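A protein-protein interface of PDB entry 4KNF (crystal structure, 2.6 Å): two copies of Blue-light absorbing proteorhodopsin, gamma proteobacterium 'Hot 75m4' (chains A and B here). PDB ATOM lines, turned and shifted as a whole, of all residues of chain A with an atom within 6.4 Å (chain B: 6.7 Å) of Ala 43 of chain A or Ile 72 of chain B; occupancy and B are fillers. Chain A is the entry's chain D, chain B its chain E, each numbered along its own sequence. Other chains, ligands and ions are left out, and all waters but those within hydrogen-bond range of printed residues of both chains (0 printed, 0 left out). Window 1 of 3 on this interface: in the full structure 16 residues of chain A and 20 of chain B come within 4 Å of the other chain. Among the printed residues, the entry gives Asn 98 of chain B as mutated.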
ATOM      1  N   THR A  38      15.601   3.189 -18.240  1.00  0.00           N
ATOM      2  CA  THR A  38      15.808   4.174 -17.191  1.00  0.00           C
ATOM      3  C   THR A  38      14.490   4.678 -16.655  1.00  0.00           C
ATOM      4  O   THR A  38      14.277   4.641 -15.449  1.00  0.00           O
ATOM      5  CB  THR A  38      16.647   5.366 -17.697  1.00  0.00           C
ATOM      6  OG1 THR A  38      17.792   4.846 -18.359  1.00  0.00           O
ATOM      7  CG2 THR A  38      17.128   6.222 -16.564  1.00  0.00           C
ATOM      8  N   ALA A  39      13.607   5.140 -17.541  1.00  0.00           N
ATOM      9  CA  ALA A  39      12.342   5.716 -17.123  1.00  0.00           C
ATOM     10  C   ALA A  39      11.523   4.629 -16.439  1.00  0.00           C
ATOM     11  O   ALA A  39      10.832   4.890 -15.453  1.00  0.00           O
ATOM     12  CB  ALA A  39      11.586   6.271 -18.312  1.00  0.00           C
ATOM     13  N   GLY A  40      11.641   3.411 -16.957  1.00  0.00           N
ATOM     14  CA  GLY A  40      10.826   2.299 -16.534  1.00  0.00           C
ATOM     15  C   GLY A  40      11.213   1.930 -15.133  1.00  0.00           C
ATOM     16  O   GLY A  40      10.352   1.738 -14.281  1.00  0.00           O
ATOM     17  N   MET A  41      12.511   1.853 -14.879  1.00  0.00           N
ATOM     18  CA  MET A  41      12.965   1.582 -13.517  1.00  0.00           C
ATOM     19  C   MET A  41      12.492   2.700 -12.592  1.00  0.00           C
ATOM     20  O   MET A  41      11.878   2.440 -11.550  1.00  0.00           O
ATOM     21  CB  MET A  41      14.476   1.481 -13.441  1.00  0.00           C
ATOM     22  CG  MET A  41      15.118   0.508 -14.393  1.00  0.00           C
ATOM     23  SD  MET A  41      14.647  -1.199 -14.118  1.00  0.00           S
ATOM     24  CE  MET A  41      15.387  -1.543 -12.545  1.00  0.00           C
ATOM     25  N   LEU A  42      12.758   3.949 -12.976  1.00  0.00           N
ATOM     26  CA  LEU A  42      12.173   5.058 -12.216  1.00  0.00           C
ATOM     27  C   LEU A  42      10.657   4.907 -11.865  1.00  0.00           C
ATOM     28  O   LEU A  42      10.296   5.023 -10.709  1.00  0.00           O
ATOM     29  CB  LEU A  42      12.431   6.400 -12.866  1.00  0.00           C
ATOM     30  CG  LEU A  42      11.956   7.543 -11.964  1.00  0.00           C
ATOM     31  CD1 LEU A  42      12.749   7.602 -10.650  1.00  0.00           C
ATOM     32  CD2 LEU A  42      11.935   8.884 -12.705  1.00  0.00           C
ATOM     33  N   ALA A  43       9.799   4.704 -12.857  1.00  0.00           N
ATOM     34  CA  ALA A  43       8.346   4.525 -12.628  1.00  0.00           C
ATOM     35  C   ALA A  43       8.127   3.369 -11.656  1.00  0.00           C
ATOM     36  O   ALA A  43       7.607   3.568 -10.577  1.00  0.00           O
ATOM     37  CB  ALA A  43       7.591   4.300 -13.944  1.00  0.00           C
ATOM     38  N   ALA A  44       8.632   2.200 -12.033  1.00  0.00           N
ATOM     39  CA  ALA A  44       8.635   0.973 -11.240  1.00  0.00           C
ATOM     40  C   ALA A  44       8.984   1.134  -9.766  1.00  0.00           C
ATOM     41  O   ALA A  44       8.296   0.606  -8.882  1.00  0.00           O
ATOM     42  CB  ALA A  44       9.579  -0.026 -11.883  1.00  0.00           C
ATOM     43  N   THR A  45      10.058   1.841  -9.496  1.00  0.00           N
ATOM     44  CA  THR A  45      10.490   2.064  -8.119  1.00  0.00           C
ATOM     45  C   THR A  45       9.417   2.787  -7.342  1.00  0.00           C
ATOM     46  O   THR A  45       9.130   2.422  -6.201  1.00  0.00           O
ATOM     47  CB  THR A  45      11.743   2.940  -8.079  1.00  0.00           C
ATOM     48  OG1 THR A  45      12.723   2.379  -8.956  1.00  0.00           O
ATOM     49  CG2 THR A  45      12.285   2.985  -6.683  1.00  0.00           C
ATOM     50  N   VAL A  46       8.855   3.825  -7.972  1.00  0.00           N
ATOM     51  CA  VAL A  46       7.826   4.633  -7.362  1.00  0.00           C
ATOM     52  C   VAL A  46       6.605   3.728  -7.159  1.00  0.00           C
ATOM     53  O   VAL A  46       6.069   3.641  -6.067  1.00  0.00           O
ATOM     54  CB  VAL A  46       7.495   5.888  -8.199  1.00  0.00           C
ATOM     55  CG1 VAL A  46       6.377   6.673  -7.551  1.00  0.00           C
ATOM     56  CG2 VAL A  46       8.706   6.789  -8.322  1.00  0.00           C
ATOM     57  N   PHE A  47       6.218   3.017  -8.207  1.00  0.00           N
ATOM     58  CA  PHE A  47       5.107   2.093  -8.143  1.00  0.00           C
ATOM     59  C   PHE A  47       5.237   1.137  -6.946  1.00  0.00           C
ATOM     60  O   PHE A  47       4.332   1.085  -6.126  1.00  0.00           O
ATOM     61  CB  PHE A  47       4.894   1.331  -9.485  1.00  0.00           C
ATOM     62  CG  PHE A  47       3.670   0.423  -9.468  1.00  0.00           C
ATOM     63  CD1 PHE A  47       2.414   0.917  -9.779  1.00  0.00           C
ATOM     64  CD2 PHE A  47       3.780  -0.913  -9.101  1.00  0.00           C
ATOM     65  CE1 PHE A  47       1.278   0.098  -9.722  1.00  0.00           C
ATOM     66  CE2 PHE A  47       2.647  -1.749  -9.034  1.00  0.00           C
ATOM     67  CZ  PHE A  47       1.391  -1.239  -9.353  1.00  0.00           C
ATOM     68  N   PHE A  48       6.358   0.413  -6.843  1.00  0.00           N
ATOM     69  CA  PHE A  48       6.544  -0.592  -5.777  1.00  0.00           C
ATOM     70  C   PHE A  48       6.543  -0.006  -4.402  1.00  0.00           C
ATOM     71  O   PHE A  48       5.881  -0.545  -3.510  1.00  0.00           O
ATOM     72  CB  PHE A  48       7.832  -1.410  -5.923  1.00  0.00           C
ATOM     73  CG  PHE A  48       7.892  -2.234  -7.168  1.00  0.00           C
ATOM     74  CD1 PHE A  48       6.789  -2.989  -7.573  1.00  0.00           C
ATOM     75  CD2 PHE A  48       9.057  -2.264  -7.942  1.00  0.00           C
ATOM     76  CE1 PHE A  48       6.840  -3.736  -8.736  1.00  0.00           C
ATOM     77  CE2 PHE A  48       9.110  -3.020  -9.106  1.00  0.00           C
ATOM     78  CZ  PHE A  48       7.998  -3.754  -9.498  1.00  0.00           C
ATOM     79  N   PHE A  74      17.812   1.900 -11.680  1.00  0.00           N
ATOM     80  CA  PHE A  74      17.659   3.266 -12.179  1.00  0.00           C
ATOM     81  C   PHE A  74      18.995   4.095 -12.198  1.00  0.00           C
ATOM     82  O   PHE A  74      19.390   4.629 -13.240  1.00  0.00           O
ATOM     83  CB  PHE A  74      16.568   3.999 -11.422  1.00  0.00           C
ATOM     84  CG  PHE A  74      16.564   5.484 -11.674  1.00  0.00           C
ATOM     85  CD1 PHE A  74      15.993   6.013 -12.859  1.00  0.00           C
ATOM     86  CD2 PHE A  74      17.146   6.363 -10.751  1.00  0.00           C
ATOM     87  CE1 PHE A  74      15.991   7.381 -13.095  1.00  0.00           C
ATOM     88  CE2 PHE A  74      17.178   7.741 -11.005  1.00  0.00           C
ATOM     89  CZ  PHE A  74      16.607   8.251 -12.173  1.00  0.00           C
ATOM     90  N   THR B  45       1.287  15.410 -10.385  1.00  0.00           N
ATOM     91  CA  THR B  45       1.972  14.241  -9.848  1.00  0.00           C
ATOM     92  C   THR B  45       1.887  14.291  -8.317  1.00  0.00           C
ATOM     93  O   THR B  45       1.477  13.314  -7.670  1.00  0.00           O
ATOM     94  CB  THR B  45       3.440  14.218 -10.311  1.00  0.00           C
ATOM     95  OG1 THR B  45       3.477  14.395 -11.737  1.00  0.00           O
ATOM     96  CG2 THR B  45       4.107  12.920  -9.938  1.00  0.00           C
ATOM     97  N   GLY B  67      -0.440   9.424 -11.196  1.00  0.00           N
ATOM     98  CA  GLY B  67       0.748  10.119 -10.763  1.00  0.00           C
ATOM     99  C   GLY B  67       1.925   9.679 -11.613  1.00  0.00           C
ATOM    100  O   GLY B  67       2.765  10.510 -12.012  1.00  0.00           O
ATOM    101  N   LEU B  68       1.993   8.370 -11.902  1.00  0.00           N
ATOM    102  CA  LEU B  68       3.074   7.871 -12.737  1.00  0.00           C
ATOM    103  C   LEU B  68       3.041   8.524 -14.132  1.00  0.00           C
ATOM    104  O   LEU B  68       4.070   8.994 -14.619  1.00  0.00           O
ATOM    105  CB  LEU B  68       3.067   6.341 -12.823  1.00  0.00           C
ATOM    106  CG  LEU B  68       3.663   5.529 -11.665  1.00  0.00           C
ATOM    107  CD1 LEU B  68       3.785   4.080 -12.114  1.00  0.00           C
ATOM    108  CD2 LEU B  68       5.003   6.068 -11.143  1.00  0.00           C
ATOM    109  N   ILE B  69       1.863   8.588 -14.750  1.00  0.00           N
ATOM    110  CA  ILE B  69       1.706   9.319 -16.021  1.00  0.00           C
ATOM    111  C   ILE B  69       2.198  10.778 -15.939  1.00  0.00           C
ATOM    112  O   ILE B  69       3.048  11.208 -16.747  1.00  0.00           O
ATOM    113  CB  ILE B  69       0.250   9.272 -16.543  1.00  0.00           C
ATOM    114  CG1 ILE B  69      -0.101   7.862 -17.027  1.00  0.00           C
ATOM    115  CG2 ILE B  69       0.063  10.224 -17.703  1.00  0.00           C
ATOM    116  CD1 ILE B  69      -1.562   7.508 -16.845  1.00  0.00           C
ATOM    117  N   THR B  70       1.688  11.538 -14.967  1.00  0.00           N
ATOM    118  CA  THR B  70       2.075  12.941 -14.856  1.00  0.00           C
ATOM    119  C   THR B  70       3.552  13.140 -14.492  1.00  0.00           C
ATOM    120  O   THR B  70       4.175  14.076 -15.001  1.00  0.00           O
ATOM    121  CB  THR B  70       1.177  13.695 -13.902  1.00  0.00           C
ATOM    122  OG1 THR B  70       0.973  12.880 -12.755  1.00  0.00           O
ATOM    123  CG2 THR B  70      -0.181  14.014 -14.580  1.00  0.00           C
ATOM    124  N   GLY B  71       4.096  12.223 -13.665  1.00  0.00           N
ATOM    125  CA  GLY B  71       5.501  12.158 -13.262  1.00  0.00           C
ATOM    126  C   GLY B  71       6.443  11.927 -14.439  1.00  0.00           C
ATOM    127  O   GLY B  71       7.421  12.677 -14.645  1.00  0.00           O
ATOM    128  N   ILE B  72       6.161  10.905 -15.244  1.00  0.00           N
ATOM    129  CA  ILE B  72       6.934  10.744 -16.471  1.00  0.00           C
ATOM    130  C   ILE B  72       6.812  11.981 -17.392  1.00  0.00           C
ATOM    131  O   ILE B  72       7.832  12.558 -17.841  1.00  0.00           O
ATOM    132  CB  ILE B  72       6.575   9.436 -17.187  1.00  0.00           C
ATOM    133  CG1 ILE B  72       7.050   8.252 -16.326  1.00  0.00           C
ATOM    134  CG2 ILE B  72       7.185   9.384 -18.598  1.00  0.00           C
ATOM    135  CD1 ILE B  72       6.304   6.973 -16.619  1.00  0.00           C
ATOM    136  N   ALA B  73       5.577  12.419 -17.634  1.00  0.00           N
ATOM    137  CA  ALA B  73       5.370  13.624 -18.439  1.00  0.00           C
ATOM    138  C   ALA B  73       6.240  14.825 -18.017  1.00  0.00           C
ATOM    139  O   ALA B  73       6.857  15.468 -18.888  1.00  0.00           O
ATOM    140  CB  ALA B  73       3.912  14.012 -18.429  1.00  0.00           C
ATOM    141  N   PHE B  74       6.266  15.124 -16.698  1.00  0.00           N
ATOM    142  CA  PHE B  74       7.074  16.202 -16.126  1.00  0.00           C
ATOM    143  C   PHE B  74       8.564  16.171 -16.543  1.00  0.00           C
ATOM    144  O   PHE B  74       9.093  17.150 -17.097  1.00  0.00           O
ATOM    145  CB  PHE B  74       6.963  16.148 -14.612  1.00  0.00           C
ATOM    146  CG  PHE B  74       8.032  16.930 -13.881  1.00  0.00           C
ATOM    147  CD1 PHE B  74       7.934  18.302 -13.746  1.00  0.00           C
ATOM    148  CD2 PHE B  74       9.112  16.272 -13.299  1.00  0.00           C
ATOM    149  CE1 PHE B  74       8.906  19.016 -13.053  1.00  0.00           C
ATOM    150  CE2 PHE B  74      10.096  16.979 -12.624  1.00  0.00           C
ATOM    151  CZ  PHE B  74       9.994  18.357 -12.492  1.00  0.00           C
ATOM    152  N   TRP B  75       9.228  15.051 -16.248  1.00  0.00           N
ATOM    153  CA  TRP B  75      10.607  14.846 -16.618  1.00  0.00           C
ATOM    154  C   TRP B  75      10.785  15.044 -18.107  1.00  0.00           C
ATOM    155  O   TRP B  75      11.739  15.749 -18.538  1.00  0.00           O
ATOM    156  CB  TRP B  75      11.119  13.474 -16.149  1.00  0.00           C
ATOM    157  CG  TRP B  75      11.321  13.433 -14.665  1.00  0.00           C
ATOM    158  CD1 TRP B  75      10.581  12.745 -13.750  1.00  0.00           C
ATOM    159  CD2 TRP B  75      12.317  14.139 -13.923  1.00  0.00           C
ATOM    160  NE1 TRP B  75      11.056  12.973 -12.478  1.00  0.00           N
ATOM    161  CE2 TRP B  75      12.117  13.833 -12.554  1.00  0.00           C
ATOM    162  CE3 TRP B  75      13.362  14.998 -14.280  1.00  0.00           C
ATOM    163  CZ2 TRP B  75      12.922  14.360 -11.541  1.00  0.00           C
ATOM    164  CZ3 TRP B  75      14.170  15.521 -13.261  1.00  0.00           C
ATOM    165  CH2 TRP B  75      13.940  15.195 -11.909  1.00  0.00           C
ATOM    166  N   HIS B  76       9.866  14.473 -18.897  1.00  0.00           N
ATOM    167  CA  HIS B  76       9.910  14.715 -20.354  1.00  0.00           C
ATOM    168  C   HIS B  76       9.674  16.160 -20.787  1.00  0.00           C
ATOM    169  O   HIS B  76      10.402  16.677 -21.653  1.00  0.00           O
ATOM    170  CB  HIS B  76       9.096  13.691 -21.139  1.00  0.00           C
ATOM    171  CG  HIS B  76       9.763  12.355 -21.160  1.00  0.00           C
ATOM    172  ND1 HIS B  76       9.606  11.435 -20.149  1.00  0.00           N
ATOM    173  CD2 HIS B  76      10.695  11.840 -21.994  1.00  0.00           C
ATOM    174  CE1 HIS B  76      10.363  10.385 -20.392  1.00  0.00           C
ATOM    175  NE2 HIS B  76      11.036  10.606 -21.503  1.00  0.00           N
ATOM    176  N   TYR B  77       8.727  16.830 -20.131  1.00  0.00           N
ATOM    177  CA  TYR B  77       8.484  18.249 -20.411  1.00  0.00           C
ATOM    178  C   TYR B  77       9.683  19.169 -20.107  1.00  0.00           C
ATOM    179  O   TYR B  77       9.826  20.247 -20.688  1.00  0.00           O
ATOM    180  CB  TYR B  77       7.218  18.731 -19.701  1.00  0.00           C
ATOM    181  CG  TYR B  77       6.013  18.652 -20.600  1.00  0.00           C
ATOM    182  CD1 TYR B  77       5.239  17.487 -20.678  1.00  0.00           C
ATOM    183  CD2 TYR B  77       5.652  19.733 -21.395  1.00  0.00           C
ATOM    184  CE1 TYR B  77       4.146  17.413 -21.522  1.00  0.00           C
ATOM    185  CE2 TYR B  77       4.558  19.666 -22.244  1.00  0.00           C
ATOM    186  CZ  TYR B  77       3.808  18.508 -22.295  1.00  0.00           C
ATOM    187  OH  TYR B  77       2.721  18.457 -23.136  1.00  0.00           O
ATOM    188  N   ILE B  97       8.741   9.571 -27.274  1.00  0.00           N
ATOM    189  CA  ILE B  97       9.235   8.790 -26.132  1.00  0.00           C
ATOM    190  C   ILE B  97       8.380   8.981 -24.859  1.00  0.00           C
ATOM    191  O   ILE B  97       8.054   7.992 -24.170  1.00  0.00           O
ATOM    192  CB  ILE B  97      10.730   9.035 -25.876  1.00  0.00           C
ATOM    193  CG1 ILE B  97      11.544   7.936 -26.550  1.00  0.00           C
ATOM    194  CG2 ILE B  97      11.051   8.993 -24.402  1.00  0.00           C
ATOM    195  CD1 ILE B  97      11.408   7.893 -28.058  1.00  0.00           C
ATOM    196  N   ASN B  98       7.972  10.225 -24.584  1.00  0.00           N
ATOM    197  CA  ASN B  98       7.059  10.481 -23.495  1.00  0.00           C
ATOM    198  C   ASN B  98       5.726   9.731 -23.662  1.00  0.00           C
ATOM    199  O   ASN B  98       5.270   9.080 -22.740  1.00  0.00           O
ATOM    200  CB  ASN B  98       6.823  11.983 -23.280  1.00  0.00           C
ATOM    201  CG  ASN B  98       5.877  12.260 -22.097  1.00  0.00           C
ATOM    202  OD1 ASN B  98       5.900  11.555 -21.083  1.00  0.00           O
ATOM    203  ND2 ASN B  98       5.027  13.270 -22.237  1.00  0.00           N
ATOM    204  N   TRP B  99       5.138   9.834 -24.858  1.00  0.00           N
ATOM    205  CA  TRP B  99       3.931   9.111 -25.255  1.00  0.00           C
ATOM    206  C   TRP B  99       4.041   7.583 -25.235  1.00  0.00           C
ATOM    207  O   TRP B  99       3.114   6.889 -24.768  1.00  0.00           O
ATOM    208  CB  TRP B  99       3.487   9.588 -26.626  1.00  0.00           C
ATOM    209  CG  TRP B  99       2.977  10.981 -26.598  1.00  0.00           C
ATOM    210  CD1 TRP B  99       2.641  11.708 -25.498  1.00  0.00           C
ATOM    211  CD2 TRP B  99       2.670  11.803 -27.731  1.00  0.00           C
ATOM    212  NE1 TRP B  99       2.162  12.945 -25.866  1.00  0.00           N
ATOM    213  CE2 TRP B  99       2.174  13.032 -27.233  1.00  0.00           C
ATOM    214  CE3 TRP B  99       2.780  11.629 -29.118  1.00  0.00           C
ATOM    215  CZ2 TRP B  99       1.790  14.082 -28.076  1.00  0.00           C
ATOM    216  CZ3 TRP B  99       2.395  12.672 -29.954  1.00  0.00           C
ATOM    217  CH2 TRP B  99       1.899  13.878 -29.433  1.00  0.00           C
ATOM    218  N   LEU B 101       5.924   5.907 -23.237  1.00  0.00           N
ATOM    219  CA  LEU B 101       5.852   5.504 -21.820  1.00  0.00           C
ATOM    220  C   LEU B 101       4.445   5.687 -21.175  1.00  0.00           C
ATOM    221  O   LEU B 101       4.034   4.891 -20.310  1.00  0.00           O
ATOM    222  CB  LEU B 101       6.935   6.199 -21.004  1.00  0.00           C
ATOM    223  CG  LEU B 101       8.361   5.751 -21.384  1.00  0.00           C
ATOM    224  CD1 LEU B 101       9.430   6.864 -21.249  1.00  0.00           C
ATOM    225  CD2 LEU B 101       8.750   4.473 -20.651  1.00  0.00           C
ATOM    226  N   THR B 102       3.708   6.713 -21.608  1.00  0.00           N
ATOM    227  CA  THR B 102       2.538   7.125 -20.879  1.00  0.00           C
ATOM    228  C   THR B 102       1.243   6.494 -21.398  1.00  0.00           C
ATOM    229  O   THR B 102       0.347   6.185 -20.598  1.00  0.00           O
ATOM    230  CB  THR B 102       2.409   8.658 -20.868  1.00  0.00           C
ATOM    231  OG1 THR B 102       2.634   9.148 -22.189  1.00  0.00           O
ATOM    232  CG2 THR B 102       3.440   9.301 -19.912  1.00  0.00           C
ATOM    233  N   LEU B 105       0.414   3.133 -20.076  1.00  0.00           N
ATOM    234  CA  LEU B 105      -0.104   3.367 -18.719  1.00  0.00           C
ATOM    235  C   LEU B 105      -1.575   3.823 -18.680  1.00  0.00           C
ATOM    236  O   LEU B 105      -2.361   3.297 -17.877  1.00  0.00           O
ATOM    237  CB  LEU B 105       0.796   4.351 -17.945  1.00  0.00           C
ATOM    238  CG  LEU B 105       2.113   3.827 -17.335  1.00  0.00           C
ATOM    239  CD1 LEU B 105       3.009   4.967 -16.870  1.00  0.00           C
ATOM    240  CD2 LEU B 105       1.842   2.869 -16.186  1.00  0.00           C
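Positions printed for both chains: 45 and 74.
The backbone carbonyl oxygen (O) of Ile 72 of chain B sits at hydrogen-bond distance from a ring nitrogen (ND1) of His 76 of chain B.
Of the printed residues of chain B, Ala 39 of chain A touches Leu 101 (3.7 Å). Printed residues of chain B within 4 Å of Ala 43 of chain A: Leu 68 (3.7 Å) and Ile 72 (3.99 Å). Of the printed residues of chain B, Val 46 of chain A touches Leu 68. Of the printed residues of chain B, Phe 47 of chain A touches Leu 68 (3.96 Å). Of the printed residues of chain A, Leu 68 of chain B touches Ala 43, Val 46 and Phe 47. Printed residues of chain A within 4 Å of Leu 101 of chain B: Ala 39. The nearest printed residue of chain A that does not touch Ile 72 of chain B is Ala 39 of chain A (5.1 Å). The nearest printed residue of chain B that does not touch Val 46 of chain A is Gly 67 of chain B (6.7 Å).
Among the printed residues, merely in contact across the chains: Ala 39 of chain A with Leu 101 of chain B, Ala 43 of chain A with Leu 68 of chain B, Ala 43 of chain A with Ile 72 of chain B, Val 46 of chain A with Leu 68 of chain B and Phe 47 of chain A with Leu 68 of chain B.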
